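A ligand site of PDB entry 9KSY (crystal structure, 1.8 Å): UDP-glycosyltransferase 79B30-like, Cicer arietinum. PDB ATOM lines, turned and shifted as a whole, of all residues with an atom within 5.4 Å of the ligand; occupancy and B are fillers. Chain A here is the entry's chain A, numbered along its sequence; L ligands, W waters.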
ATOM      1  N   MET A  17       7.369 -11.955 -17.819  1.00  0.00           N
ATOM      2  CA  MET A  17       7.152 -11.203 -16.589  1.00  0.00           C
ATOM      3  C   MET A  17       6.738 -12.147 -15.455  1.00  0.00           C
ATOM      4  O   MET A  17       7.086 -11.916 -14.290  1.00  0.00           O
ATOM      5  CB  MET A  17       6.077 -10.142 -16.815  1.00  0.00           C
ATOM      6  CG  MET A  17       6.545  -9.097 -17.822  1.00  0.00           C
ATOM      7  SD  MET A  17       7.948  -8.147 -17.262  1.00  0.00           S
ATOM      8  CE  MET A  17       7.367  -7.517 -15.687  1.00  0.00           C
ATOM      9  N   GLY A  18       6.062 -13.241 -15.797  1.00  0.00           N
ATOM     10  CA  GLY A  18       5.644 -14.217 -14.795  1.00  0.00           C
ATOM     11  C   GLY A  18       6.768 -15.070 -14.251  1.00  0.00           C
ATOM     12  O   GLY A  18       6.543 -15.833 -13.301  1.00  0.00           O
ATOM     13  N   ILE A  21       9.186 -11.712 -12.183  1.00  0.00           N
ATOM     14  CA  ILE A  21       8.620 -11.103 -10.976  1.00  0.00           C
ATOM     15  C   ILE A  21       8.803 -12.037  -9.775  1.00  0.00           C
ATOM     16  O   ILE A  21       9.279 -11.584  -8.719  1.00  0.00           O
ATOM     17  CB  ILE A  21       7.158 -10.698 -11.202  1.00  0.00           C
ATOM     18  CG1 ILE A  21       7.087  -9.415 -12.046  1.00  0.00           C
ATOM     19  CG2 ILE A  21       6.436 -10.553  -9.882  1.00  0.00           C
ATOM     20  CD1 ILE A  21       5.691  -9.126 -12.597  1.00  0.00           C
ATOM     21  N   LEU A 272      -6.185 -12.045 -17.431  1.00  0.00           N
ATOM     22  CA  LEU A 272      -5.647 -13.299 -17.968  1.00  0.00           C
ATOM     23  C   LEU A 272      -4.149 -13.175 -18.248  1.00  0.00           C
ATOM     24  O   LEU A 272      -3.630 -13.698 -19.235  1.00  0.00           O
ATOM     25  CB  LEU A 272      -6.418 -13.712 -19.224  1.00  0.00           C
ATOM     26  CG  LEU A 272      -7.956 -13.695 -19.081  1.00  0.00           C
ATOM     27  CD1 LEU A 272      -8.642 -14.146 -20.384  1.00  0.00           C
ATOM     28  CD2 LEU A 272      -8.410 -14.574 -17.937  1.00  0.00           C
ATOM     29  N   GLY A 273      -3.442 -12.465 -17.368  1.00  0.00           N
ATOM     30  CA  GLY A 273      -1.992 -12.395 -17.460  1.00  0.00           C
ATOM     31  C   GLY A 273      -1.545 -11.418 -18.526  1.00  0.00           C
ATOM     32  O   GLY A 273      -2.323 -10.633 -19.074  1.00  0.00           O
ATOM     33  N   SER A 274      -0.258 -11.503 -18.854  1.00  0.00           N
ATOM     34  CA  SER A 274       0.410 -10.530 -19.708  1.00  0.00           C
ATOM     35  C   SER A 274       0.805 -11.079 -21.061  1.00  0.00           C
ATOM     36  O   SER A 274       1.446 -10.361 -21.840  1.00  0.00           O
ATOM     37  CB  SER A 274       1.690 -10.015 -19.023  1.00  0.00           C
ATOM     38  OG  SER A 274       2.621 -11.091 -18.873  1.00  0.00           O
ATOM     39  N   GLU A 275       0.470 -12.331 -21.379  1.00  0.00           N
ATOM     40  CA  GLU A 275       0.971 -12.946 -22.600  1.00  0.00           C
ATOM     41  C   GLU A 275      -0.095 -13.189 -23.646  1.00  0.00           C
ATOM     42  O   GLU A 275       0.154 -12.970 -24.826  1.00  0.00           O
ATOM     43  CB  GLU A 275       1.680 -14.269 -22.289  1.00  0.00           C
ATOM     44  CG  GLU A 275       2.821 -14.180 -21.281  1.00  0.00           C
ATOM     45  CD  GLU A 275       3.423 -15.550 -21.009  1.00  0.00           C
ATOM     46  OE1 GLU A 275       4.661 -15.710 -21.175  1.00  0.00           O
ATOM     47  OE2 GLU A 275       2.671 -16.480 -20.611  1.00  0.00           O
ATOM     48  N   ILE A 300      -8.903  -6.717 -17.438  1.00  0.00           N
ATOM     49  CA  ILE A 300      -7.591  -6.389 -17.973  1.00  0.00           C
ATOM     50  C   ILE A 300      -7.311  -7.421 -19.070  1.00  0.00           C
ATOM     51  O   ILE A 300      -6.931  -8.550 -18.778  1.00  0.00           O
ATOM     52  CB  ILE A 300      -6.512  -6.397 -16.881  1.00  0.00           C
ATOM     53  CG1 ILE A 300      -6.956  -5.520 -15.715  1.00  0.00           C
ATOM     54  CG2 ILE A 300      -5.150  -5.985 -17.451  1.00  0.00           C
ATOM     55  CD1 ILE A 300      -7.244  -4.082 -16.115  1.00  0.00           C
ATOM     56  N   GLY A 331      -3.841  -2.092 -20.959  1.00  0.00           N
ATOM     57  CA  GLY A 331      -2.468  -1.873 -20.522  1.00  0.00           C
ATOM     58  C   GLY A 331      -2.051  -2.704 -19.295  1.00  0.00           C
ATOM     59  O   GLY A 331      -2.859  -3.334 -18.613  1.00  0.00           O
ATOM     60  N   TRP A 332      -0.735  -2.694 -19.034  1.00  0.00           N
ATOM     61  CA  TRP A 332      -0.184  -3.253 -17.799  1.00  0.00           C
ATOM     62  C   TRP A 332      -0.674  -2.454 -16.592  1.00  0.00           C
ATOM     63  O   TRP A 332      -0.611  -1.221 -16.582  1.00  0.00           O
ATOM     64  CB  TRP A 332       1.339  -3.217 -17.861  1.00  0.00           C
ATOM     65  CG  TRP A 332       2.017  -3.738 -16.636  1.00  0.00           C
ATOM     66  CD1 TRP A 332       2.371  -3.025 -15.520  1.00  0.00           C
ATOM     67  CD2 TRP A 332       2.460  -5.077 -16.429  1.00  0.00           C
ATOM     68  NE1 TRP A 332       3.002  -3.869 -14.612  1.00  0.00           N
ATOM     69  CE2 TRP A 332       3.066  -5.131 -15.160  1.00  0.00           C
ATOM     70  CE3 TRP A 332       2.401  -6.249 -17.194  1.00  0.00           C
ATOM     71  CZ2 TRP A 332       3.594  -6.298 -14.639  1.00  0.00           C
ATOM     72  CZ3 TRP A 332       2.925  -7.404 -16.668  1.00  0.00           C
ATOM     73  CH2 TRP A 332       3.524  -7.417 -15.401  1.00  0.00           C
ATOM     74  N   ILE A 333      -1.163  -3.149 -15.553  1.00  0.00           N
ATOM     75  CA  ILE A 333      -1.561  -2.460 -14.332  1.00  0.00           C
ATOM     76  C   ILE A 333      -0.892  -3.134 -13.139  1.00  0.00           C
ATOM     77  O   ILE A 333      -0.211  -4.147 -13.268  1.00  0.00           O
ATOM     78  CB  ILE A 333      -3.098  -2.390 -14.164  1.00  0.00           C
ATOM     79  CG1 ILE A 333      -3.789  -3.697 -14.583  1.00  0.00           C
ATOM     80  CG2 ILE A 333      -3.652  -1.244 -14.981  1.00  0.00           C
ATOM     81  CD1 ILE A 333      -3.492  -4.872 -13.727  1.00  0.00           C
ATOM     82  N   GLN A 334      -1.075  -2.525 -11.962  1.00  0.00           N
ATOM     83  CA  GLN A 334      -0.463  -3.069 -10.735  1.00  0.00           C
ATOM     84  C   GLN A 334      -1.410  -4.103 -10.130  1.00  0.00           C
ATOM     85  O   GLN A 334      -2.141  -3.840  -9.173  1.00  0.00           O
ATOM     86  CB  GLN A 334      -0.154  -1.931  -9.763  1.00  0.00           C
ATOM     87  CG  GLN A 334       0.798  -0.889 -10.334  1.00  0.00           C
ATOM     88  CD  GLN A 334       0.724   0.422  -9.584  1.00  0.00           C
ATOM     89  OE1 GLN A 334      -0.170   1.219  -9.828  1.00  0.00           O
ATOM     90  NE2 GLN A 334       1.670   0.647  -8.656  1.00  0.00           N
ATOM     91  N   GLN A 335      -1.379  -5.324 -10.680  1.00  0.00           N
ATOM     92  CA  GLN A 335      -2.381  -6.328 -10.311  1.00  0.00           C
ATOM     93  C   GLN A 335      -2.340  -6.637  -8.821  1.00  0.00           C
ATOM     94  O   GLN A 335      -3.383  -6.740  -8.169  1.00  0.00           O
ATOM     95  CB  GLN A 335      -2.196  -7.610 -11.127  1.00  0.00           C
ATOM     96  CG  GLN A 335      -3.044  -8.767 -10.605  1.00  0.00           C
ATOM     97  CD  GLN A 335      -3.128  -9.919 -11.585  1.00  0.00           C
ATOM     98  OE1 GLN A 335      -3.695  -9.766 -12.670  1.00  0.00           O
ATOM     99  NE2 GLN A 335      -2.539 -11.064 -11.229  1.00  0.00           N
ATOM    100  N   GLN A 336      -1.151  -6.819  -8.269  1.00  0.00           N
ATOM    101  CA  GLN A 336      -1.058  -7.199  -6.867  1.00  0.00           C
ATOM    102  C   GLN A 336      -1.706  -6.126  -5.983  1.00  0.00           C
ATOM    103  O   GLN A 336      -2.383  -6.453  -5.006  1.00  0.00           O
ATOM    104  CB  GLN A 336       0.407  -7.437  -6.483  1.00  0.00           C
ATOM    105  CG  GLN A 336       0.688  -7.465  -4.987  1.00  0.00           C
ATOM    106  CD  GLN A 336       2.165  -7.332  -4.672  1.00  0.00           C
ATOM    107  OE1 GLN A 336       3.023  -7.582  -5.524  1.00  0.00           O
ATOM    108  NE2 GLN A 336       2.475  -6.912  -3.464  1.00  0.00           N
ATOM    109  N   HIS A 350      -6.903 -16.516 -15.175  1.00  0.00           N
ATOM    110  CA  HIS A 350      -6.451 -17.539 -16.118  1.00  0.00           C
ATOM    111  C   HIS A 350      -5.648 -18.639 -15.441  1.00  0.00           C
ATOM    112  O   HIS A 350      -5.230 -19.591 -16.126  1.00  0.00           O
ATOM    113  CB  HIS A 350      -5.633 -16.907 -17.260  1.00  0.00           C
ATOM    114  CG  HIS A 350      -4.226 -16.526 -16.892  1.00  0.00           C
ATOM    115  ND1 HIS A 350      -3.906 -15.839 -15.746  1.00  0.00           N
ATOM    116  CD2 HIS A 350      -3.056 -16.743 -17.550  1.00  0.00           C
ATOM    117  CE1 HIS A 350      -2.597 -15.631 -15.712  1.00  0.00           C
ATOM    118  NE2 HIS A 350      -2.066 -16.162 -16.804  1.00  0.00           N
ATOM    119  N   GLY A 352      -2.667 -18.580 -14.074  1.00  0.00           N
ATOM    120  CA  GLY A 352      -1.216 -18.480 -13.983  1.00  0.00           C
ATOM    121  C   GLY A 352      -0.765 -18.618 -12.537  1.00  0.00           C
ATOM    122  O   GLY A 352      -1.441 -18.160 -11.602  1.00  0.00           O
ATOM    123  N   ALA A 353       0.396 -19.254 -12.342  1.00  0.00           N
ATOM    124  CA  ALA A 353       0.857 -19.555 -10.991  1.00  0.00           C
ATOM    125  C   ALA A 353       1.056 -18.303 -10.146  1.00  0.00           C
ATOM    126  O   ALA A 353       0.821 -18.328  -8.931  1.00  0.00           O
ATOM    127  CB  ALA A 353       2.154 -20.361 -11.054  1.00  0.00           C
ATOM    128  N   GLY A 354       1.494 -17.206 -10.760  1.00  0.00           N
ATOM    129  CA  GLY A 354       1.700 -15.984  -9.999  1.00  0.00           C
ATOM    130  C   GLY A 354       0.379 -15.360  -9.582  1.00  0.00           C
ATOM    131  O   GLY A 354       0.194 -14.961  -8.419  1.00  0.00           O
ATOM    132  N   SER A 355      -0.560 -15.285 -10.525  1.00  0.00           N
ATOM    133  CA  SER A 355      -1.888 -14.762 -10.235  1.00  0.00           C
ATOM    134  C   SER A 355      -2.594 -15.604  -9.178  1.00  0.00           C
ATOM    135  O   SER A 355      -3.306 -15.048  -8.327  1.00  0.00           O
ATOM    136  CB  SER A 355      -2.719 -14.713 -11.524  1.00  0.00           C
ATOM    137  OG  SER A 355      -2.185 -13.742 -12.427  1.00  0.00           O
ATOM    138  N   ILE A 356      -2.414 -16.928  -9.211  1.00  0.00           N
ATOM    139  CA  ILE A 356      -3.015 -17.797  -8.194  1.00  0.00           C
ATOM    140  C   ILE A 356      -2.517 -17.413  -6.800  1.00  0.00           C
ATOM    141  O   ILE A 356      -3.310 -17.255  -5.871  1.00  0.00           O
ATOM    142  CB  ILE A 356      -2.715 -19.281  -8.486  1.00  0.00           C
ATOM    143  CG1 ILE A 356      -3.601 -19.811  -9.633  1.00  0.00           C
ATOM    144  CG2 ILE A 356      -2.993 -20.166  -7.250  1.00  0.00           C
ATOM    145  CD1 ILE A 356      -5.088 -19.664  -9.358  1.00  0.00           C
ATOM    146  N   GLU A 358      -1.294 -14.565  -5.822  1.00  0.00           N
ATOM    147  CA  GLU A 358      -1.812 -13.245  -5.496  1.00  0.00           C
ATOM    148  C   GLU A 358      -3.276 -13.280  -5.095  1.00  0.00           C
ATOM    149  O   GLU A 358      -3.699 -12.512  -4.219  1.00  0.00           O
ATOM    150  CB  GLU A 358      -1.566 -12.297  -6.679  1.00  0.00           C
ATOM    151  CG  GLU A 358      -0.071 -12.119  -6.858  1.00  0.00           C
ATOM    152  CD  GLU A 358       0.362 -11.555  -8.205  1.00  0.00           C
ATOM    153  OE1 GLU A 358      -0.499 -11.141  -9.017  1.00  0.00           O
ATOM    154  OE2 GLU A 358       1.586 -11.516  -8.429  1.00  0.00           O
ATOM    155  N   TYR A 376      -1.733 -23.809 -16.431  1.00  0.00           N
ATOM    156  CA  TYR A 376      -3.006 -23.174 -16.100  1.00  0.00           C
ATOM    157  C   TYR A 376      -4.066 -24.230 -15.812  1.00  0.00           C
ATOM    158  O   TYR A 376      -4.856 -24.101 -14.873  1.00  0.00           O
ATOM    159  CB  TYR A 376      -3.516 -22.278 -17.225  1.00  0.00           C
ATOM    160  CG  TYR A 376      -2.546 -21.187 -17.686  1.00  0.00           C
ATOM    161  CD1 TYR A 376      -1.491 -20.771 -16.886  1.00  0.00           C
ATOM    162  CD2 TYR A 376      -2.717 -20.581 -18.934  1.00  0.00           C
ATOM    163  CE1 TYR A 376      -0.617 -19.777 -17.332  1.00  0.00           C
ATOM    164  CE2 TYR A 376      -1.854 -19.604 -19.372  1.00  0.00           C
ATOM    165  CZ  TYR A 376      -0.817 -19.210 -18.570  1.00  0.00           C
ATOM    166  OH  TYR A 376       0.038 -18.229 -19.036  1.00  0.00           O
HETATM  167  N1  LIG L   1       0.761  -8.734 -13.864  1.00  0.00           N
HETATM  168  C1  LIG L   1       0.693  -7.389 -13.528  1.00  0.00           C
HETATM  169  N2  LIG L   1      -0.046  -6.621 -14.402  1.00  0.00           N
HETATM  170  C2  LIG L   1      -0.690  -7.039 -15.551  1.00  0.00           C
HETATM  171  C3  LIG L   1      -0.557  -8.444 -15.826  1.00  0.00           C
HETATM  172  C4  LIG L   1       0.165  -9.220 -14.995  1.00  0.00           C
HETATM  173  O1  LIG L   1       1.210  -6.917 -12.531  1.00  0.00           O
HETATM  174  O2  LIG L   1      -1.300  -6.218 -16.224  1.00  0.00           O
HETATM  175  C5  LIG L   1       1.588  -9.601 -12.998  1.00  0.00           C
HETATM  176  C6  LIG L   1       0.798 -10.514 -12.062  1.00  0.00           C
HETATM  177  O3  LIG L   1       0.458  -9.800 -10.885  1.00  0.00           O
HETATM  178  C7  LIG L   1       1.807 -11.651 -11.859  1.00  0.00           C
HETATM  179  C8  LIG L   1       2.451 -11.754 -13.259  1.00  0.00           C
HETATM  180  O4  LIG L   1       2.312 -10.447 -13.856  1.00  0.00           O
HETATM  181  O5  LIG L   1       2.780 -11.303 -10.897  1.00  0.00           O
HETATM  182  C9  LIG L   1       1.782 -12.723 -14.191  1.00  0.00           C
HETATM  183  O6  LIG L   1       2.221 -14.040 -13.851  1.00  0.00           O
HETATM  184  P1  LIG L   1       1.189 -15.241 -14.048  1.00  0.00           P
HETATM  185  O7  LIG L   1      -0.032 -15.016 -13.213  1.00  0.00           O
HETATM  186  O8  LIG L   1       1.956 -16.491 -13.842  1.00  0.00           O
HETATM  187  O9  LIG L   1       0.681 -15.050 -15.569  1.00  0.00           O
HETATM  188  P2  LIG L   1       1.309 -14.788 -17.045  1.00  0.00           P
HETATM  189  O10 LIG L   1       2.737 -15.301 -16.953  1.00  0.00           O
HETATM  190  O11 LIG L   1       1.224 -13.266 -17.304  1.00  0.00           O
HETATM  191  O12 LIG L   1       0.442 -15.569 -17.969  1.00  0.00           O
HETATM  192  O   HOH W   1       4.289 -13.706 -10.350  1.00  0.00           O
HETATM  193  O   HOH W   2       4.691 -13.874 -18.203  1.00  0.00           O
HETATM  194  O   HOH W   3       4.281 -16.076 -11.986  1.00  0.00           O
HETATM  195  O   HOH W   4      -1.014 -14.455 -20.089  1.00  0.00           O
HETATM  196  O   HOH W   5       4.830 -16.994 -18.183  1.00  0.00           O
HETATM  197  O   HOH W   6      -1.685  -6.611 -19.391  1.00  0.00           O
HETATM  198  O   HOH W   7       2.149 -18.216 -15.881  1.00  0.00           O
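N of Ser 355 lies within hydrogen-bond range of O7 of the ligand, at 2.8 Å.
The side-chain hydroxyl (OH) of Tyr 376 sits at hydrogen-bond distance from an oxygen (O12) of the ligand (2.9 Å).
O11 of the ligand lies within hydrogen-bond range of N of Ser 274.
The backbone NH of Gly 354 is in hydrogen-bond range of an oxygen (O8) of the ligand (3.2 Å).
A ring nitrogen (NE2) of His 350 lies within hydrogen-bond range of an oxygen (O12) of the ligand (2.8 Å).
The side-chain hydroxyl (OG) of Ser 274 lies within hydrogen-bond range of an oxygen (O11) of the ligand.
O3 of the ligand is in hydrogen-bond range of OE1 of Glu 358.
NE2 of Gln 335 is in hydrogen-bond range of O3 of the ligand, 3.3 Å away.
The backbone carbonyl oxygen of Ile 333 is in hydrogen-bond range of a nitrogen (N2) of the ligand, at 2.7 Å.
O7 of the ligand sits at hydrogen-bond distance from OG of Ser 355 (2.6 Å).
N of Ile 333 lies within hydrogen-bond range of O2 of the ligand (3.1 Å).
ND1 of His 350 sits close to N of Gly 352, 3.4 Å away.
The side-chain hydroxyl of Ser 355 is in hydrogen-bond range of the side-chain amide nitrogen of Gln 335.
OE1 of Glu 358 is in hydrogen-bond range of NE2 of Gln 335 (3.0 Å).
Merely in contact with the ligand: Trp 332, Gly 273, Ala 353, Gly 18, Glu 275, Gly 352 and Ile 21.
Hydrophobic or aromatic side chains that line the ligand: Ile 21, Trp 332, Ile 333, His 350 and Tyr 376.
15 residues have an atom within 4 Å of the ligand: Gly 18, Ile 21, Gly 273, Ser 274, Glu 275, Trp 332, Ile 333, Gln 335, His 350, Gly 352, Ala 353, Gly 354, Ser 355, Glu 358 and Tyr 376.
The nearest printed residue that does not touch the ligand is Ile 300 (4.05 Å).
Water W2 lies within hydrogen-bond range of an oxygen (O10) of the ligand (2.7 Å), the backbone NH (N) of Gly 18 (2.8 Å), the backbone NH (N) of Met 17 (3.3 Å) and the side-chain carboxylate (OE1) of Glu 275 (3.5 Å).
Water W4 lies within hydrogen-bond range of O12 of the ligand, O of Leu 272, N of Glu 275 and N of Ser 274.
Water W5 bridges O10 of the ligand (3.0 Å) and OE1 of Glu 275 (3.3 Å).
Water W3 lies within hydrogen-bond range of the backbone carbonyl oxygen (O) of Gly 18, an oxygen (O8) of the ligand and the backbone NH (N) of Gly 354.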
